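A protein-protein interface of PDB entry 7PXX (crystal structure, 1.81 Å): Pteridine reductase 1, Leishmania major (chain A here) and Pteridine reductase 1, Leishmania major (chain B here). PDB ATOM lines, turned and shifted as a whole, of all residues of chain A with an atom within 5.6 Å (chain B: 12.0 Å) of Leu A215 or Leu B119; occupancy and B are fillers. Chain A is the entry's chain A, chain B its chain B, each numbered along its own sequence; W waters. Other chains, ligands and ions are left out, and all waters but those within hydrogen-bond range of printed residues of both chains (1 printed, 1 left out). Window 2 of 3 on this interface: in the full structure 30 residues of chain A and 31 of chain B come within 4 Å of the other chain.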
ATOM      1  N   ALA A 159      32.377  23.579 -10.016  1.00  0.00           N
ATOM      2  CA  ALA A 159      32.577  23.668  -8.569  1.00  0.00           C
ATOM      3  C   ALA A 159      32.925  22.309  -7.973  1.00  0.00           C
ATOM      4  O   ALA A 159      33.795  22.203  -7.094  1.00  0.00           O
ATOM      5  CB  ALA A 159      31.320  24.236  -7.904  1.00  0.00           C
ATOM      6  N   HIS A 160      32.248  21.254  -8.446  1.00  0.00           N
ATOM      7  CA  HIS A 160      32.520  19.903  -7.969  1.00  0.00           C
ATOM      8  C   HIS A 160      33.965  19.490  -8.211  1.00  0.00           C
ATOM      9  O   HIS A 160      34.595  18.888  -7.334  1.00  0.00           O
ATOM     10  CB  HIS A 160      31.563  18.916  -8.638  1.00  0.00           C
ATOM     11  CG  HIS A 160      30.256  18.797  -7.925  1.00  0.00           C
ATOM     12  ND1 HIS A 160      29.612  17.593  -7.733  1.00  0.00           N
ATOM     13  CD2 HIS A 160      29.490  19.733  -7.318  1.00  0.00           C
ATOM     14  CE1 HIS A 160      28.497  17.796  -7.053  1.00  0.00           C
ATOM     15  NE2 HIS A 160      28.403  19.086  -6.787  1.00  0.00           N
ATOM     16  N   VAL A 162      36.587  21.441  -8.555  1.00  0.00           N
ATOM     17  CA  VAL A 162      37.466  22.189  -7.659  1.00  0.00           C
ATOM     18  C   VAL A 162      37.419  21.607  -6.251  1.00  0.00           C
ATOM     19  O   VAL A 162      38.464  21.340  -5.639  1.00  0.00           O
ATOM     20  CB  VAL A 162      37.110  23.682  -7.649  1.00  0.00           C
ATOM     21  CG1 VAL A 162      37.986  24.403  -6.567  1.00  0.00           C
ATOM     22  CG2 VAL A 162      37.266  24.285  -9.047  1.00  0.00           C
ATOM     23  N   ALA A 163      36.209  21.405  -5.712  1.00  0.00           N
ATOM     24  CA  ALA A 163      36.077  20.828  -4.378  1.00  0.00           C
ATOM     25  C   ALA A 163      36.806  19.493  -4.266  1.00  0.00           C
ATOM     26  O   ALA A 163      37.366  19.170  -3.210  1.00  0.00           O
ATOM     27  CB  ALA A 163      34.602  20.657  -4.017  1.00  0.00           C
ATOM     28  N   ARG A 170      45.006  23.118  -5.943  1.00  0.00           N
ATOM     29  CA  ARG A 170      43.986  23.945  -6.574  1.00  0.00           C
ATOM     30  C   ARG A 170      44.634  25.115  -7.307  1.00  0.00           C
ATOM     31  O   ARG A 170      45.729  25.556  -6.961  1.00  0.00           O
ATOM     32  CB  ARG A 170      42.980  24.446  -5.533  1.00  0.00           C
ATOM     33  CG  ARG A 170      41.909  23.425  -5.196  1.00  0.00           C
ATOM     34  CD  ARG A 170      41.150  23.789  -3.903  1.00  0.00           C
ATOM     35  NE  ARG A 170      40.321  22.663  -3.472  1.00  0.00           N
ATOM     36  CZ  ARG A 170      39.692  22.574  -2.310  1.00  0.00           C
ATOM     37  NH1 ARG A 170      39.774  23.554  -1.423  1.00  0.00           N
ATOM     38  NH2 ARG A 170      38.968  21.496  -2.045  1.00  0.00           N
ATOM     39  N   TYR A 174      40.238  31.190  -9.701  1.00  0.00           N
ATOM     40  CA  TYR A 174      39.065  30.605 -10.347  1.00  0.00           C
ATOM     41  C   TYR A 174      38.054  31.702 -10.635  1.00  0.00           C
ATOM     42  O   TYR A 174      37.747  32.515  -9.758  1.00  0.00           O
ATOM     43  CB  TYR A 174      38.397  29.566  -9.448  1.00  0.00           C
ATOM     44  CG  TYR A 174      39.164  28.298  -9.285  1.00  0.00           C
ATOM     45  CD1 TYR A 174      39.297  27.413 -10.341  1.00  0.00           C
ATOM     46  CD2 TYR A 174      39.737  27.970  -8.060  1.00  0.00           C
ATOM     47  CE1 TYR A 174      39.995  26.251 -10.197  1.00  0.00           C
ATOM     48  CE2 TYR A 174      40.438  26.799  -7.904  1.00  0.00           C
ATOM     49  CZ  TYR A 174      40.565  25.942  -8.964  1.00  0.00           C
ATOM     50  OH  TYR A 174      41.267  24.768  -8.792  1.00  0.00           O
ATOM     51  N   GLU A 211      27.605  31.024  -2.669  1.00  0.00           N
ATOM     52  CA  GLU A 211      27.870  29.653  -2.240  1.00  0.00           C
ATOM     53  C   GLU A 211      29.293  29.210  -2.561  1.00  0.00           C
ATOM     54  O   GLU A 211      29.850  28.373  -1.838  1.00  0.00           O
ATOM     55  CB  GLU A 211      26.874  28.693  -2.878  1.00  0.00           C
ATOM     56  CG  GLU A 211      27.013  27.262  -2.420  1.00  0.00           C
ATOM     57  CD  GLU A 211      25.761  26.463  -2.721  1.00  0.00           C
ATOM     58  OE1 GLU A 211      24.918  26.984  -3.484  1.00  0.00           O
ATOM     59  OE2 GLU A 211      25.612  25.339  -2.202  1.00  0.00           O
ATOM     60  N   LEU A 212      29.912  29.749  -3.619  1.00  0.00           N
ATOM     61  CA  LEU A 212      31.258  29.312  -3.981  1.00  0.00           C
ATOM     62  C   LEU A 212      32.354  30.242  -3.479  1.00  0.00           C
ATOM     63  O   LEU A 212      33.538  29.960  -3.704  1.00  0.00           O
ATOM     64  CB  LEU A 212      31.392  29.140  -5.501  1.00  0.00           C
ATOM     65  CG  LEU A 212      30.320  28.219  -6.099  1.00  0.00           C
ATOM     66  CD1 LEU A 212      30.604  28.009  -7.565  1.00  0.00           C
ATOM     67  CD2 LEU A 212      30.251  26.897  -5.323  1.00  0.00           C
ATOM     68  N   ALA A 213      32.007  31.334  -2.813  1.00  0.00           N
ATOM     69  CA  ALA A 213      33.037  32.145  -2.168  1.00  0.00           C
ATOM     70  C   ALA A 213      33.987  31.364  -1.252  1.00  0.00           C
ATOM     71  O   ALA A 213      35.184  31.702  -1.232  1.00  0.00           O
ATOM     72  CB  ALA A 213      32.381  33.304  -1.390  1.00  0.00           C
ATOM     73  N   PRO A 214      33.556  30.368  -0.466  1.00  0.00           N
ATOM     74  CA  PRO A 214      34.540  29.646   0.366  1.00  0.00           C
ATOM     75  C   PRO A 214      35.649  28.981  -0.436  1.00  0.00           C
ATOM     76  O   PRO A 214      36.777  28.883   0.053  1.00  0.00           O
ATOM     77  CB  PRO A 214      33.689  28.598   1.105  1.00  0.00           C
ATOM     78  CG  PRO A 214      32.325  29.143   1.120  1.00  0.00           C
ATOM     79  CD  PRO A 214      32.176  29.919  -0.172  1.00  0.00           C
ATOM     80  N   LEU A 215      35.377  28.520  -1.653  1.00  0.00           N
ATOM     81  CA  LEU A 215      36.436  27.970  -2.484  1.00  0.00           C
ATOM     82  C   LEU A 215      37.109  29.026  -3.346  1.00  0.00           C
ATOM     83  O   LEU A 215      37.808  28.676  -4.302  1.00  0.00           O
ATOM     84  CB  LEU A 215      35.885  26.865  -3.376  1.00  0.00           C
ATOM     85  CG  LEU A 215      35.433  25.619  -2.650  1.00  0.00           C
ATOM     86  CD1 LEU A 215      34.492  24.854  -3.556  1.00  0.00           C
ATOM     87  CD2 LEU A 215      36.672  24.796  -2.295  1.00  0.00           C
ATOM     88  N   GLN A 216      36.899  30.308  -3.043  1.00  0.00           N
ATOM     89  CA  GLN A 216      37.539  31.404  -3.769  1.00  0.00           C
ATOM     90  C   GLN A 216      37.200  31.356  -5.258  1.00  0.00           C
ATOM     91  O   GLN A 216      37.975  31.815  -6.091  1.00  0.00           O
ATOM     92  CB  GLN A 216      39.060  31.408  -3.544  1.00  0.00           C
ATOM     93  CG  GLN A 216      39.446  31.423  -2.036  1.00  0.00           C
ATOM     94  CD  GLN A 216      40.852  31.933  -1.771  1.00  0.00           C
ATOM     95  OE1 GLN A 216      41.637  32.146  -2.695  1.00  0.00           O
ATOM     96  NE2 GLN A 216      41.176  32.130  -0.505  1.00  0.00           N
ATOM     97  N   ILE A 217      36.042  30.799  -5.602  1.00  0.00           N
ATOM     98  CA  ILE A 217      35.525  30.850  -6.970  1.00  0.00           C
ATOM     99  C   ILE A 217      34.642  32.082  -7.075  1.00  0.00           C
ATOM    100  O   ILE A 217      33.584  32.156  -6.440  1.00  0.00           O
ATOM    101  CB  ILE A 217      34.744  29.589  -7.350  1.00  0.00           C
ATOM    102  CG1 ILE A 217      35.645  28.351  -7.315  1.00  0.00           C
ATOM    103  CG2 ILE A 217      34.112  29.736  -8.784  1.00  0.00           C
ATOM    104  CD1 ILE A 217      34.849  27.062  -7.393  1.00  0.00           C
ATOM    105  N   TYR B 114      13.018  24.335  -1.932  1.00  0.00           N
ATOM    106  CA  TYR B 114      13.907  23.489  -1.140  1.00  0.00           C
ATOM    107  C   TYR B 114      15.319  23.626  -1.707  1.00  0.00           C
ATOM    108  O   TYR B 114      15.490  24.102  -2.838  1.00  0.00           O
ATOM    109  CB  TYR B 114      13.433  22.013  -1.137  1.00  0.00           C
ATOM    110  CG  TYR B 114      13.041  21.481  -2.497  1.00  0.00           C
ATOM    111  CD1 TYR B 114      14.002  21.011  -3.391  1.00  0.00           C
ATOM    112  CD2 TYR B 114      11.711  21.464  -2.898  1.00  0.00           C
ATOM    113  CE1 TYR B 114      13.655  20.547  -4.633  1.00  0.00           C
ATOM    114  CE2 TYR B 114      11.349  20.991  -4.143  1.00  0.00           C
ATOM    115  CZ  TYR B 114      12.331  20.551  -5.007  1.00  0.00           C
ATOM    116  OH  TYR B 114      11.966  20.107  -6.243  1.00  0.00           O
ATOM    117  N   PRO B 115      16.349  23.238  -0.948  1.00  0.00           N
ATOM    118  CA  PRO B 115      17.727  23.483  -1.397  1.00  0.00           C
ATOM    119  C   PRO B 115      18.089  22.677  -2.631  1.00  0.00           C
ATOM    120  O   PRO B 115      17.645  21.538  -2.809  1.00  0.00           O
ATOM    121  CB  PRO B 115      18.584  23.033  -0.203  1.00  0.00           C
ATOM    122  CG  PRO B 115      17.667  22.994   0.952  1.00  0.00           C
ATOM    123  CD  PRO B 115      16.311  22.706   0.427  1.00  0.00           C
ATOM    124  N   THR B 116      18.915  23.296  -3.488  1.00  0.00           N
ATOM    125  CA  THR B 116      19.627  22.615  -4.573  1.00  0.00           C
ATOM    126  C   THR B 116      21.098  22.991  -4.466  1.00  0.00           C
ATOM    127  O   THR B 116      21.582  23.860  -5.212  1.00  0.00           O
ATOM    128  CB  THR B 116      19.103  23.013  -5.945  1.00  0.00           C
ATOM    129  OG1 THR B 116      19.108  24.434  -6.057  1.00  0.00           O
ATOM    130  CG2 THR B 116      17.699  22.471  -6.181  1.00  0.00           C
ATOM    131  N   PRO B 117      21.834  22.380  -3.538  1.00  0.00           N
ATOM    132  CA  PRO B 117      23.200  22.846  -3.256  1.00  0.00           C
ATOM    133  C   PRO B 117      24.131  22.642  -4.437  1.00  0.00           C
ATOM    134  O   PRO B 117      24.017  21.668  -5.192  1.00  0.00           O
ATOM    135  CB  PRO B 117      23.637  21.979  -2.067  1.00  0.00           C
ATOM    136  CG  PRO B 117      22.387  21.417  -1.507  1.00  0.00           C
ATOM    137  CD  PRO B 117      21.445  21.268  -2.663  1.00  0.00           C
ATOM    138  N   LEU B 118      25.086  23.568  -4.572  1.00  0.00           N
ATOM    139  CA  LEU B 118      26.143  23.401  -5.561  1.00  0.00           C
ATOM    140  C   LEU B 118      27.216  22.445  -5.061  1.00  0.00           C
ATOM    141  O   LEU B 118      27.772  21.684  -5.847  1.00  0.00           O
ATOM    142  CB  LEU B 118      26.747  24.763  -5.921  1.00  0.00           C
ATOM    143  CG  LEU B 118      25.757  25.664  -6.650  1.00  0.00           C
ATOM    144  CD1 LEU B 118      26.370  27.017  -6.955  1.00  0.00           C
ATOM    145  CD2 LEU B 118      25.251  24.989  -7.936  1.00  0.00           C
ATOM    146  N   LEU B 119      27.492  22.443  -3.761  1.00  0.00           N
ATOM    147  CA  LEU B 119      28.544  21.615  -3.183  1.00  0.00           C
ATOM    148  C   LEU B 119      27.938  20.438  -2.436  1.00  0.00           C
ATOM    149  O   LEU B 119      26.898  20.580  -1.787  1.00  0.00           O
ATOM    150  CB  LEU B 119      29.422  22.436  -2.242  1.00  0.00           C
ATOM    151  CG  LEU B 119      30.043  23.623  -2.963  1.00  0.00           C
ATOM    152  CD1 LEU B 119      30.460  24.769  -2.009  1.00  0.00           C
ATOM    153  CD2 LEU B 119      31.198  23.129  -3.830  1.00  0.00           C
ATOM    154  N   ARG B 120      28.614  19.290  -2.516  1.00  0.00           N
ATOM    155  CA  ARG B 120      28.126  17.998  -2.011  1.00  0.00           C
ATOM    156  C   ARG B 120      27.625  18.047  -0.572  1.00  0.00           C
ATOM    157  O   ARG B 120      28.296  18.578   0.309  1.00  0.00           O
ATOM    158  CB  ARG B 120      29.237  16.942  -2.130  1.00  0.00           C
ATOM    159  N   MET B 136      18.373  15.534  -9.041  1.00  0.00           N
ATOM    160  CA  MET B 136      18.684  16.793  -9.709  1.00  0.00           C
ATOM    161  C   MET B 136      17.749  17.038 -10.889  1.00  0.00           C
ATOM    162  O   MET B 136      17.318  18.177 -11.118  1.00  0.00           O
ATOM    163  CB  MET B 136      20.142  16.806 -10.163  1.00  0.00           C
ATOM    164  CG  MET B 136      21.095  17.446  -9.162  1.00  0.00           C
ATOM    165  SD  MET B 136      20.524  19.045  -8.544  1.00  0.00           S
ATOM    166  CE  MET B 136      20.242  19.941 -10.057  1.00  0.00           C
ATOM    167  N   LEU B 188      19.495  33.077  -0.673  1.00  0.00           N
ATOM    168  CA  LEU B 188      19.554  32.143   0.435  1.00  0.00           C
ATOM    169  C   LEU B 188      20.524  31.033   0.067  1.00  0.00           C
ATOM    170  O   LEU B 188      20.410  30.434  -1.009  1.00  0.00           O
ATOM    171  CB  LEU B 188      18.157  31.595   0.722  1.00  0.00           C
ATOM    172  CG  LEU B 188      17.878  30.744   1.961  1.00  0.00           C
ATOM    173  CD1 LEU B 188      18.119  31.518   3.247  1.00  0.00           C
ATOM    174  CD2 LEU B 188      16.433  30.253   1.888  1.00  0.00           C
ATOM    175  N   LEU B 189      21.510  30.797   0.933  1.00  0.00           N
ATOM    176  CA  LEU B 189      22.589  29.861   0.631  1.00  0.00           C
ATOM    177  C   LEU B 189      22.047  28.467   0.322  1.00  0.00           C
ATOM    178  O   LEU B 189      21.306  27.889   1.123  1.00  0.00           O
ATOM    179  CB  LEU B 189      23.553  29.802   1.814  1.00  0.00           C
ATOM    180  CG  LEU B 189      24.832  28.993   1.590  1.00  0.00           C
ATOM    181  CD1 LEU B 189      25.798  29.777   0.698  1.00  0.00           C
ATOM    182  CD2 LEU B 189      25.495  28.630   2.897  1.00  0.00           C
ATOM    183  N   GLY B 190      22.414  27.934  -0.843  1.00  0.00           N
ATOM    184  CA  GLY B 190      22.051  26.583  -1.206  1.00  0.00           C
ATOM    185  C   GLY B 190      20.743  26.445  -1.947  1.00  0.00           C
ATOM    186  O   GLY B 190      20.317  25.309  -2.195  1.00  0.00           O
ATOM    187  N   TYR B 191      20.113  27.560  -2.344  1.00  0.00           N
ATOM    188  CA  TYR B 191      18.823  27.536  -3.031  1.00  0.00           C
ATOM    189  C   TYR B 191      18.907  28.075  -4.451  1.00  0.00           C
ATOM    190  O   TYR B 191      18.082  28.913  -4.853  1.00  0.00           O
ATOM    191  CB  TYR B 191      17.796  28.352  -2.257  1.00  0.00           C
ATOM    192  CG  TYR B 191      17.305  27.689  -0.992  1.00  0.00           C
ATOM    193  CD1 TYR B 191      18.100  27.614   0.142  1.00  0.00           C
ATOM    194  CD2 TYR B 191      16.035  27.142  -0.938  1.00  0.00           C
ATOM    195  CE1 TYR B 191      17.638  27.009   1.298  1.00  0.00           C
ATOM    196  CE2 TYR B 191      15.570  26.535   0.206  1.00  0.00           C
ATOM    197  CZ  TYR B 191      16.370  26.471   1.314  1.00  0.00           C
ATOM    198  OH  TYR B 191      15.867  25.859   2.437  1.00  0.00           O
ATOM    199  N   THR B 192      19.862  27.573  -5.233  1.00  0.00           N
ATOM    200  CA  THR B 192      20.186  28.250  -6.481  1.00  0.00           C
ATOM    201  C   THR B 192      19.050  28.154  -7.482  1.00  0.00           C
ATOM    202  O   THR B 192      18.643  29.169  -8.038  1.00  0.00           O
ATOM    203  CB  THR B 192      21.497  27.728  -7.050  1.00  0.00           C
ATOM    204  OG1 THR B 192      22.547  28.127  -6.155  1.00  0.00           O
ATOM    205  CG2 THR B 192      21.770  28.365  -8.385  1.00  0.00           C
ATOM    206  N   ILE B 193      18.486  26.955  -7.685  1.00  0.00           N
ATOM    207  CA  ILE B 193      17.412  26.804  -8.671  1.00  0.00           C
ATOM    208  C   ILE B 193      16.211  27.677  -8.320  1.00  0.00           C
ATOM    209  O   ILE B 193      15.612  28.331  -9.194  1.00  0.00           O
ATOM    210  CB  ILE B 193      17.000  25.329  -8.808  1.00  0.00           C
ATOM    211  CG1 ILE B 193      18.187  24.494  -9.274  1.00  0.00           C
ATOM    212  CG2 ILE B 193      15.878  25.222  -9.803  1.00  0.00           C
ATOM    213  CD1 ILE B 193      18.285  24.412 -10.783  1.00  0.00           C
HETATM  214  O   HOH W   1      23.530  29.722  -2.821  1.00  0.00           O
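No residue of chain B comes within 4 Å of Ala A159. His A160 touches just one residue of chain B: Leu B118 (2.8 Å). No residue of chain B comes within 4 Å of Ala A163. No residue of chain B comes within 4 Å of Tyr A174. Glu A211 touches just these residues of chain B: Pro B117 (3.6 Å), Leu B118 (3.0 Å), Leu B119 (3.7 Å), Leu B189 (3.6 Å), Gly B190 (3.7 Å) and Thr B192 (3.7 Å). No residue of chain B comes within 4 Å of Ala A213. Pro A214 touches none of the printed residues of chain B. Leu A215 touches just one residue of chain B: Leu B119 (3.7 Å). No residue of chain B comes within 4 Å of Gln A216. No residue of chain B comes within 4 Å of Ile A217. Printed residues of chain A within 4 Å of Pro B117: Glu A211. Of the printed residues of chain A, Gly B190 touches Glu A211. Of the printed residues of chain A, Thr B192 touches Glu A211. The nearest printed residue of chain A that does not touch Leu B119 is Ala A163 (4.2 Å). The nearest printed residue of chain A that does not touch Thr B192 is Leu A212 (7.8 Å).
Among the printed residues, merely in contact across the chains: Glu A211 with Leu B189, Glu A211 with Pro B117, Glu A211 with Leu B119, Glu A211 with Gly B190, Leu A215 with Leu B119, Glu A211 with Thr B192 and Leu A212 with Leu B119.
Water W1 bridges N of Gly B190 (2.9 Å) and OE1 of Glu A211 (3.1 Å).
The backbone NH of Leu B118 lies within hydrogen-bond range of the side-chain carboxylate of Glu A211. The backbone carbonyl oxygen (O) of Leu B118 sits at hydrogen-bond distance from a ring nitrogen (NE2) of His A160, at 2.8 Å.
Hydrophobic or aromatic side chains of chain B that line the printed part of chain A: Pro B117, Leu B118, Leu B119 and Leu B189. Of the 13 printed residues of chain A, 4 touch a printed residue of chain B. Hydrophobic or aromatic side chains of chain A within 4 Å of the printed part of chain B: His A160, Leu A212 and Leu A215. Among the printed residues, 9 pairs touch across the chains.
The backbone carbonyl oxygen (O) of Gly B190 lies within hydrogen-bond range of the backbone NH (N) of Thr B116. N of Ile A217 lies within hydrogen-bond range of O of Leu A212, at 3.3 Å. The side-chain hydroxyl (OG1) of Thr B116 lies within hydrogen-bond range of the backbone NH (N) of Thr B192 (3.3 Å).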
